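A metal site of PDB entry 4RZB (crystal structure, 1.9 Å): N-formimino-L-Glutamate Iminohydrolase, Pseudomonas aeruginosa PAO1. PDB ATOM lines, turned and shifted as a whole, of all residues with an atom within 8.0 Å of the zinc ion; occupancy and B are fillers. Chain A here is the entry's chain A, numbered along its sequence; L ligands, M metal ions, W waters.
The side-chain carboxylate (OD2) of Asp 320 lies within salt-bridge range of a nitrogen (N2) of the ligand (3.7 Å). OH of Tyr 121 sits at hydrogen-bond distance from O1 of the ligand, 2.6 Å away. The side-chain carboxylate (OE2) of Glu 235 is in salt-bridge range of a nitrogen (N2) of the ligand (3.0 Å). The side-chain amide nitrogen (NE2) of Gln 61 sits at hydrogen-bond distance from an oxygen (O1) of the ligand, 3.0 Å away. NE2 of His 206 is in hydrogen-bond range of O2 of the ligand (2.7 Å).
The backbone carbonyl oxygen (O) of Phe 119 is in hydrogen-bond range of a ring nitrogen (ND1) of His 58 (2.9 Å). The backbone NH (N) of Ser 319 is in hydrogen-bond range of the backbone carbonyl oxygen (O) of His 56, 3.2 Å away. ND1 of His 232 lies within hydrogen-bond range of O of His 206, at 2.9 Å.
Water W1 lies within hydrogen-bond range of the side-chain carboxylate of Asp 320, a ring nitrogen (NE2) of His 269 and a nitrogen (N2) of the ligand.
The zinc ion is bound by water W1 (2.0 Å), NE2 of His 58 (2.0 Å), NE2 of His 56 (2.1 Å), NE2 of His 232 (2.2 Å) and OD1 of Asp 320 (2.5 Å).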
ATOM      1  N   HIS A  56     -19.549  20.499 -30.780  1.00  0.00           N
ATOM      2  CA  HIS A  56     -18.971  21.723 -30.198  1.00  0.00           C
ATOM      3  C   HIS A  56     -19.009  21.705 -28.674  1.00  0.00           C
ATOM      4  O   HIS A  56     -20.091  21.659 -28.083  1.00  0.00           O
ATOM      5  CB  HIS A  56     -19.693  22.973 -30.734  1.00  0.00           C
ATOM      6  CG  HIS A  56     -19.030  24.265 -30.351  1.00  0.00           C
ATOM      7  ND1 HIS A  56     -17.797  24.647 -30.863  1.00  0.00           N
ATOM      8  CD2 HIS A  56     -19.418  25.263 -29.523  1.00  0.00           C
ATOM      9  CE1 HIS A  56     -17.469  25.825 -30.358  1.00  0.00           C
ATOM     10  NE2 HIS A  56     -18.428  26.221 -29.546  1.00  0.00           N
ATOM     11  N   SER A  57     -17.838  21.757 -28.046  1.00  0.00           N
ATOM     12  CA  SER A  57     -17.698  21.710 -26.596  1.00  0.00           C
ATOM     13  C   SER A  57     -16.544  22.574 -26.073  1.00  0.00           C
ATOM     14  O   SER A  57     -15.449  22.545 -26.623  1.00  0.00           O
ATOM     15  CB  SER A  57     -17.388  20.264 -26.181  1.00  0.00           C
ATOM     16  OG  SER A  57     -17.010  20.209 -24.814  1.00  0.00           O
ATOM     17  N   HIS A  58     -16.788  23.332 -24.987  1.00  0.00           N
ATOM     18  CA  HIS A  58     -15.693  23.882 -24.174  1.00  0.00           C
ATOM     19  C   HIS A  58     -15.786  23.286 -22.786  1.00  0.00           C
ATOM     20  O   HIS A  58     -16.532  23.804 -21.937  1.00  0.00           O
ATOM     21  CB  HIS A  58     -15.748  25.407 -24.071  1.00  0.00           C
ATOM     22  CG  HIS A  58     -16.041  26.099 -25.365  1.00  0.00           C
ATOM     23  ND1 HIS A  58     -15.207  26.014 -26.465  1.00  0.00           N
ATOM     24  CD2 HIS A  58     -17.060  26.915 -25.736  1.00  0.00           C
ATOM     25  CE1 HIS A  58     -15.706  26.740 -27.447  1.00  0.00           C
ATOM     26  NE2 HIS A  58     -16.829  27.288 -27.037  1.00  0.00           N
ATOM     27  N   GLN A  61     -16.329  24.784 -19.113  1.00  0.00           N
ATOM     28  CA  GLN A  61     -17.475  25.635 -18.845  1.00  0.00           C
ATOM     29  C   GLN A  61     -18.574  24.901 -18.074  1.00  0.00           C
ATOM     30  O   GLN A  61     -19.404  25.520 -17.409  1.00  0.00           O
ATOM     31  CB  GLN A  61     -18.008  26.256 -20.143  1.00  0.00           C
ATOM     32  CG  GLN A  61     -17.034  27.308 -20.712  1.00  0.00           C
ATOM     33  CD  GLN A  61     -17.555  28.016 -21.948  1.00  0.00           C
ATOM     34  OE1 GLN A  61     -18.740  27.912 -22.282  1.00  0.00           O
ATOM     35  NE2 GLN A  61     -16.665  28.746 -22.646  1.00  0.00           N
ATOM     36  N   PHE A  78     -24.432  38.817 -23.206  1.00  0.00           N
ATOM     37  CA  PHE A  78     -23.414  37.866 -23.591  1.00  0.00           C
ATOM     38  C   PHE A  78     -22.039  38.326 -23.076  1.00  0.00           C
ATOM     39  O   PHE A  78     -21.245  37.526 -22.606  1.00  0.00           O
ATOM     40  CB  PHE A  78     -23.429  37.759 -25.117  1.00  0.00           C
ATOM     41  CG  PHE A  78     -22.329  36.922 -25.685  1.00  0.00           C
ATOM     42  CD1 PHE A  78     -22.538  35.586 -25.973  1.00  0.00           C
ATOM     43  CD2 PHE A  78     -21.092  37.491 -25.964  1.00  0.00           C
ATOM     44  CE1 PHE A  78     -21.530  34.822 -26.499  1.00  0.00           C
ATOM     45  CE2 PHE A  78     -20.076  36.725 -26.495  1.00  0.00           C
ATOM     46  CZ  PHE A  78     -20.293  35.394 -26.761  1.00  0.00           C
ATOM     47  N   TRP A  81     -21.605  37.920 -19.333  1.00  0.00           N
ATOM     48  CA  TRP A  81     -21.436  36.480 -19.105  1.00  0.00           C
ATOM     49  C   TRP A  81     -20.004  36.089 -19.420  1.00  0.00           C
ATOM     50  O   TRP A  81     -19.371  35.334 -18.681  1.00  0.00           O
ATOM     51  CB  TRP A  81     -22.378  35.646 -19.985  1.00  0.00           C
ATOM     52  CG  TRP A  81     -21.979  34.158 -20.051  1.00  0.00           C
ATOM     53  CD1 TRP A  81     -22.355  33.182 -19.184  1.00  0.00           C
ATOM     54  CD2 TRP A  81     -21.132  33.531 -21.024  1.00  0.00           C
ATOM     55  NE1 TRP A  81     -21.793  31.967 -19.558  1.00  0.00           N
ATOM     56  CE2 TRP A  81     -21.039  32.161 -20.678  1.00  0.00           C
ATOM     57  CE3 TRP A  81     -20.442  33.988 -22.156  1.00  0.00           C
ATOM     58  CZ2 TRP A  81     -20.290  31.256 -21.424  1.00  0.00           C
ATOM     59  CZ3 TRP A  81     -19.689  33.078 -22.896  1.00  0.00           C
ATOM     60  CH2 TRP A  81     -19.623  31.735 -22.525  1.00  0.00           C
ATOM     61  N   PHE A 119     -13.501  22.087 -28.710  1.00  0.00           N
ATOM     62  CA  PHE A 119     -13.053  23.358 -29.262  1.00  0.00           C
ATOM     63  C   PHE A 119     -12.224  23.968 -28.140  1.00  0.00           C
ATOM     64  O   PHE A 119     -12.730  24.681 -27.272  1.00  0.00           O
ATOM     65  CB  PHE A 119     -14.319  24.164 -29.576  1.00  0.00           C
ATOM     66  CG  PHE A 119     -14.119  25.395 -30.435  1.00  0.00           C
ATOM     67  CD1 PHE A 119     -13.532  26.536 -29.921  1.00  0.00           C
ATOM     68  CD2 PHE A 119     -14.620  25.445 -31.730  1.00  0.00           C
ATOM     69  CE1 PHE A 119     -13.400  27.693 -30.698  1.00  0.00           C
ATOM     70  CE2 PHE A 119     -14.498  26.587 -32.516  1.00  0.00           C
ATOM     71  CZ  PHE A 119     -13.888  27.715 -31.982  1.00  0.00           C
ATOM     72  N   TYR A 121      -9.407  26.030 -26.276  1.00  0.00           N
ATOM     73  CA  TYR A 121      -8.577  27.235 -26.336  1.00  0.00           C
ATOM     74  C   TYR A 121      -7.833  27.579 -25.042  1.00  0.00           C
ATOM     75  O   TYR A 121      -7.169  28.606 -24.967  1.00  0.00           O
ATOM     76  CB  TYR A 121      -9.406  28.445 -26.784  1.00  0.00           C
ATOM     77  CG  TYR A 121     -10.684  28.679 -26.007  1.00  0.00           C
ATOM     78  CD1 TYR A 121     -10.652  29.123 -24.698  1.00  0.00           C
ATOM     79  CD2 TYR A 121     -11.927  28.466 -26.603  1.00  0.00           C
ATOM     80  CE1 TYR A 121     -11.839  29.352 -23.985  1.00  0.00           C
ATOM     81  CE2 TYR A 121     -13.102  28.698 -25.909  1.00  0.00           C
ATOM     82  CZ  TYR A 121     -13.050  29.133 -24.605  1.00  0.00           C
ATOM     83  OH  TYR A 121     -14.224  29.376 -23.930  1.00  0.00           O
ATOM     84  N   HIS A 206     -10.612  30.674 -33.353  1.00  0.00           N
ATOM     85  CA  HIS A 206     -11.654  30.976 -32.367  1.00  0.00           C
ATOM     86  C   HIS A 206     -12.844  31.710 -32.992  1.00  0.00           C
ATOM     87  O   HIS A 206     -13.992  31.332 -32.768  1.00  0.00           O
ATOM     88  CB  HIS A 206     -11.127  31.784 -31.186  1.00  0.00           C
ATOM     89  CG  HIS A 206     -12.220  32.193 -30.234  1.00  0.00           C
ATOM     90  ND1 HIS A 206     -12.897  33.383 -30.352  1.00  0.00           N
ATOM     91  CD2 HIS A 206     -12.768  31.545 -29.178  1.00  0.00           C
ATOM     92  CE1 HIS A 206     -13.804  33.467 -29.391  1.00  0.00           C
ATOM     93  NE2 HIS A 206     -13.749  32.369 -28.668  1.00  0.00           N
ATOM     94  N   ILE A 231     -14.845  27.209 -36.657  1.00  0.00           N
ATOM     95  CA  ILE A 231     -14.746  28.604 -36.243  1.00  0.00           C
ATOM     96  C   ILE A 231     -16.086  29.033 -35.631  1.00  0.00           C
ATOM     97  O   ILE A 231     -17.136  28.617 -36.121  1.00  0.00           O
ATOM     98  CB  ILE A 231     -14.358  29.508 -37.461  1.00  0.00           C
ATOM     99  CG1 ILE A 231     -14.190  30.976 -37.041  1.00  0.00           C
ATOM    100  CG2 ILE A 231     -15.383  29.367 -38.597  1.00  0.00           C
ATOM    101  CD1 ILE A 231     -13.568  31.844 -38.162  1.00  0.00           C
ATOM    102  N   HIS A 232     -16.064  29.823 -34.547  1.00  0.00           N
ATOM    103  CA  HIS A 232     -17.273  30.506 -34.070  1.00  0.00           C
ATOM    104  C   HIS A 232     -17.559  31.620 -35.057  1.00  0.00           C
ATOM    105  O   HIS A 232     -16.654  32.402 -35.378  1.00  0.00           O
ATOM    106  CB  HIS A 232     -17.078  31.236 -32.721  1.00  0.00           C
ATOM    107  CG  HIS A 232     -16.939  30.350 -31.517  1.00  0.00           C
ATOM    108  ND1 HIS A 232     -15.828  30.395 -30.705  1.00  0.00           N
ATOM    109  CD2 HIS A 232     -17.792  29.483 -30.937  1.00  0.00           C
ATOM    110  CE1 HIS A 232     -15.983  29.556 -29.705  1.00  0.00           C
ATOM    111  NE2 HIS A 232     -17.173  28.984 -29.818  1.00  0.00           N
ATOM    112  N   GLU A 235     -22.300  34.751 -34.004  1.00  0.00           N
ATOM    113  CA  GLU A 235     -23.122  34.404 -32.847  1.00  0.00           C
ATOM    114  C   GLU A 235     -23.912  35.605 -32.299  1.00  0.00           C
ATOM    115  O   GLU A 235     -25.091  35.471 -31.962  1.00  0.00           O
ATOM    116  CB  GLU A 235     -22.276  33.795 -31.741  1.00  0.00           C
ATOM    117  CG  GLU A 235     -23.112  33.349 -30.539  1.00  0.00           C
ATOM    118  CD  GLU A 235     -22.299  32.729 -29.426  1.00  0.00           C
ATOM    119  OE1 GLU A 235     -21.047  32.827 -29.454  1.00  0.00           O
ATOM    120  OE2 GLU A 235     -22.906  32.140 -28.490  1.00  0.00           O
ATOM    121  N   VAL A 268     -19.677  27.423 -36.401  1.00  0.00           N
ATOM    122  CA  VAL A 268     -20.413  27.301 -35.135  1.00  0.00           C
ATOM    123  C   VAL A 268     -21.285  28.526 -34.888  1.00  0.00           C
ATOM    124  O   VAL A 268     -20.839  29.665 -35.051  1.00  0.00           O
ATOM    125  CB  VAL A 268     -19.465  27.069 -33.944  1.00  0.00           C
ATOM    126  CG1 VAL A 268     -20.268  26.715 -32.687  1.00  0.00           C
ATOM    127  CG2 VAL A 268     -18.478  25.923 -34.263  1.00  0.00           C
ATOM    128  N   HIS A 269     -22.536  28.251 -34.486  1.00  0.00           N
ATOM    129  CA  HIS A 269     -23.618  29.205 -34.300  1.00  0.00           C
ATOM    130  C   HIS A 269     -24.188  29.695 -35.629  1.00  0.00           C
ATOM    131  O   HIS A 269     -25.317  29.321 -35.996  1.00  0.00           O
ATOM    132  CB  HIS A 269     -23.215  30.378 -33.386  1.00  0.00           C
ATOM    133  CG  HIS A 269     -22.607  29.937 -32.088  1.00  0.00           C
ATOM    134  ND1 HIS A 269     -23.259  29.090 -31.210  1.00  0.00           N
ATOM    135  CD2 HIS A 269     -21.392  30.187 -31.544  1.00  0.00           C
ATOM    136  CE1 HIS A 269     -22.485  28.873 -30.166  1.00  0.00           C
ATOM    137  NE2 HIS A 269     -21.343  29.519 -30.339  1.00  0.00           N
ATOM    138  N   CYS A 291     -25.932  25.238 -31.452  1.00  0.00           N
ATOM    139  CA  CYS A 291     -25.872  24.913 -30.032  1.00  0.00           C
ATOM    140  C   CYS A 291     -27.084  25.522 -29.345  1.00  0.00           C
ATOM    141  O   CYS A 291     -26.999  26.613 -28.771  1.00  0.00           O
ATOM    142  CB  CYS A 291     -24.563  25.464 -29.444  1.00  0.00           C
ATOM    143  SG  CYS A 291     -23.080  24.884 -30.372  1.00  0.00           S
ATOM    144  N   THR A 294     -27.324  26.520 -25.374  1.00  0.00           N
ATOM    145  CA  THR A 294     -26.400  27.616 -25.073  1.00  0.00           C
ATOM    146  C   THR A 294     -26.820  28.930 -25.745  1.00  0.00           C
ATOM    147  O   THR A 294     -26.774  29.995 -25.132  1.00  0.00           O
ATOM    148  CB  THR A 294     -24.928  27.251 -25.427  1.00  0.00           C
ATOM    149  OG1 THR A 294     -24.439  26.284 -24.477  1.00  0.00           O
ATOM    150  CG2 THR A 294     -24.034  28.493 -25.354  1.00  0.00           C
ATOM    151  N   LEU A 298     -27.588  32.225 -23.690  1.00  0.00           N
ATOM    152  CA  LEU A 298     -26.803  33.435 -23.885  1.00  0.00           C
ATOM    153  C   LEU A 298     -27.579  34.544 -24.615  1.00  0.00           C
ATOM    154  O   LEU A 298     -27.048  35.660 -24.827  1.00  0.00           O
ATOM    155  CB  LEU A 298     -25.499  33.099 -24.611  1.00  0.00           C
ATOM    156  CG  LEU A 298     -24.571  32.164 -23.822  1.00  0.00           C
ATOM    157  CD1 LEU A 298     -23.285  31.892 -24.611  1.00  0.00           C
ATOM    158  CD2 LEU A 298     -24.254  32.760 -22.471  1.00  0.00           C
ATOM    159  N   SER A 319     -23.164  20.999 -27.461  1.00  0.00           N
ATOM    160  CA  SER A 319     -23.590  21.413 -26.125  1.00  0.00           C
ATOM    161  C   SER A 319     -22.838  22.651 -25.617  1.00  0.00           C
ATOM    162  O   SER A 319     -23.281  23.294 -24.656  1.00  0.00           O
ATOM    163  CB  SER A 319     -23.548  20.237 -25.131  1.00  0.00           C
ATOM    164  OG  SER A 319     -22.224  19.773 -24.890  1.00  0.00           O
ATOM    165  N   ASP A 320     -21.698  22.959 -26.239  1.00  0.00           N
ATOM    166  CA  ASP A 320     -21.030  24.283 -26.106  1.00  0.00           C
ATOM    167  C   ASP A 320     -20.638  24.679 -24.659  1.00  0.00           C
ATOM    168  O   ASP A 320     -19.623  24.223 -24.152  1.00  0.00           O
ATOM    169  CB  ASP A 320     -21.877  25.387 -26.776  1.00  0.00           C
ATOM    170  CG  ASP A 320     -21.115  26.686 -26.961  1.00  0.00           C
ATOM    171  OD1 ASP A 320     -19.892  26.712 -26.691  1.00  0.00           O
ATOM    172  OD2 ASP A 320     -21.731  27.686 -27.377  1.00  0.00           O
ATOM    173  N   SER A 321     -21.456  25.510 -24.005  1.00  0.00           N
ATOM    174  CA  SER A 321     -21.171  25.905 -22.621  1.00  0.00           C
ATOM    175  C   SER A 321     -21.646  24.845 -21.623  1.00  0.00           C
ATOM    176  O   SER A 321     -21.400  24.950 -20.420  1.00  0.00           O
ATOM    177  CB  SER A 321     -21.856  27.246 -22.301  1.00  0.00           C
ATOM    178  OG  SER A 321     -23.264  27.065 -22.170  1.00  0.00           O
HETATM  179  C1  LIG L   1     -16.145  31.131 -26.078  1.00  0.00           C
HETATM  180  N1  LIG L   1     -18.515  31.348 -26.111  1.00  0.00           N
HETATM  181  O1  LIG L   1     -16.361  30.252 -25.187  1.00  0.00           O
HETATM  182  O2  LIG L   1     -14.963  31.378 -26.427  1.00  0.00           O
HETATM  183  C2  LIG L   1     -17.294  31.862 -26.697  1.00  0.00           C
HETATM  184  C3  LIG L   1     -17.149  33.336 -26.436  1.00  0.00           C
HETATM  185  C4  LIG L   1     -19.660  31.773 -26.845  1.00  0.00           C
HETATM  186  N2  LIG L   1     -20.804  31.189 -26.553  1.00  0.00           N
HETATM  187  C5  LIG L   1     -16.598  34.154 -27.554  1.00  0.00           C
HETATM  188  O3  LIG L   1     -16.918  33.873 -28.740  1.00  0.00           O
HETATM  189  O4  LIG L   1     -15.810  35.108 -27.317  1.00  0.00           O
HETATM  190 ZN    ZN M   1     -18.298  27.852 -28.310  1.00  0.00          ZN
HETATM  191  O   HOH W   1     -19.817  29.121 -28.310  1.00  0.00           O
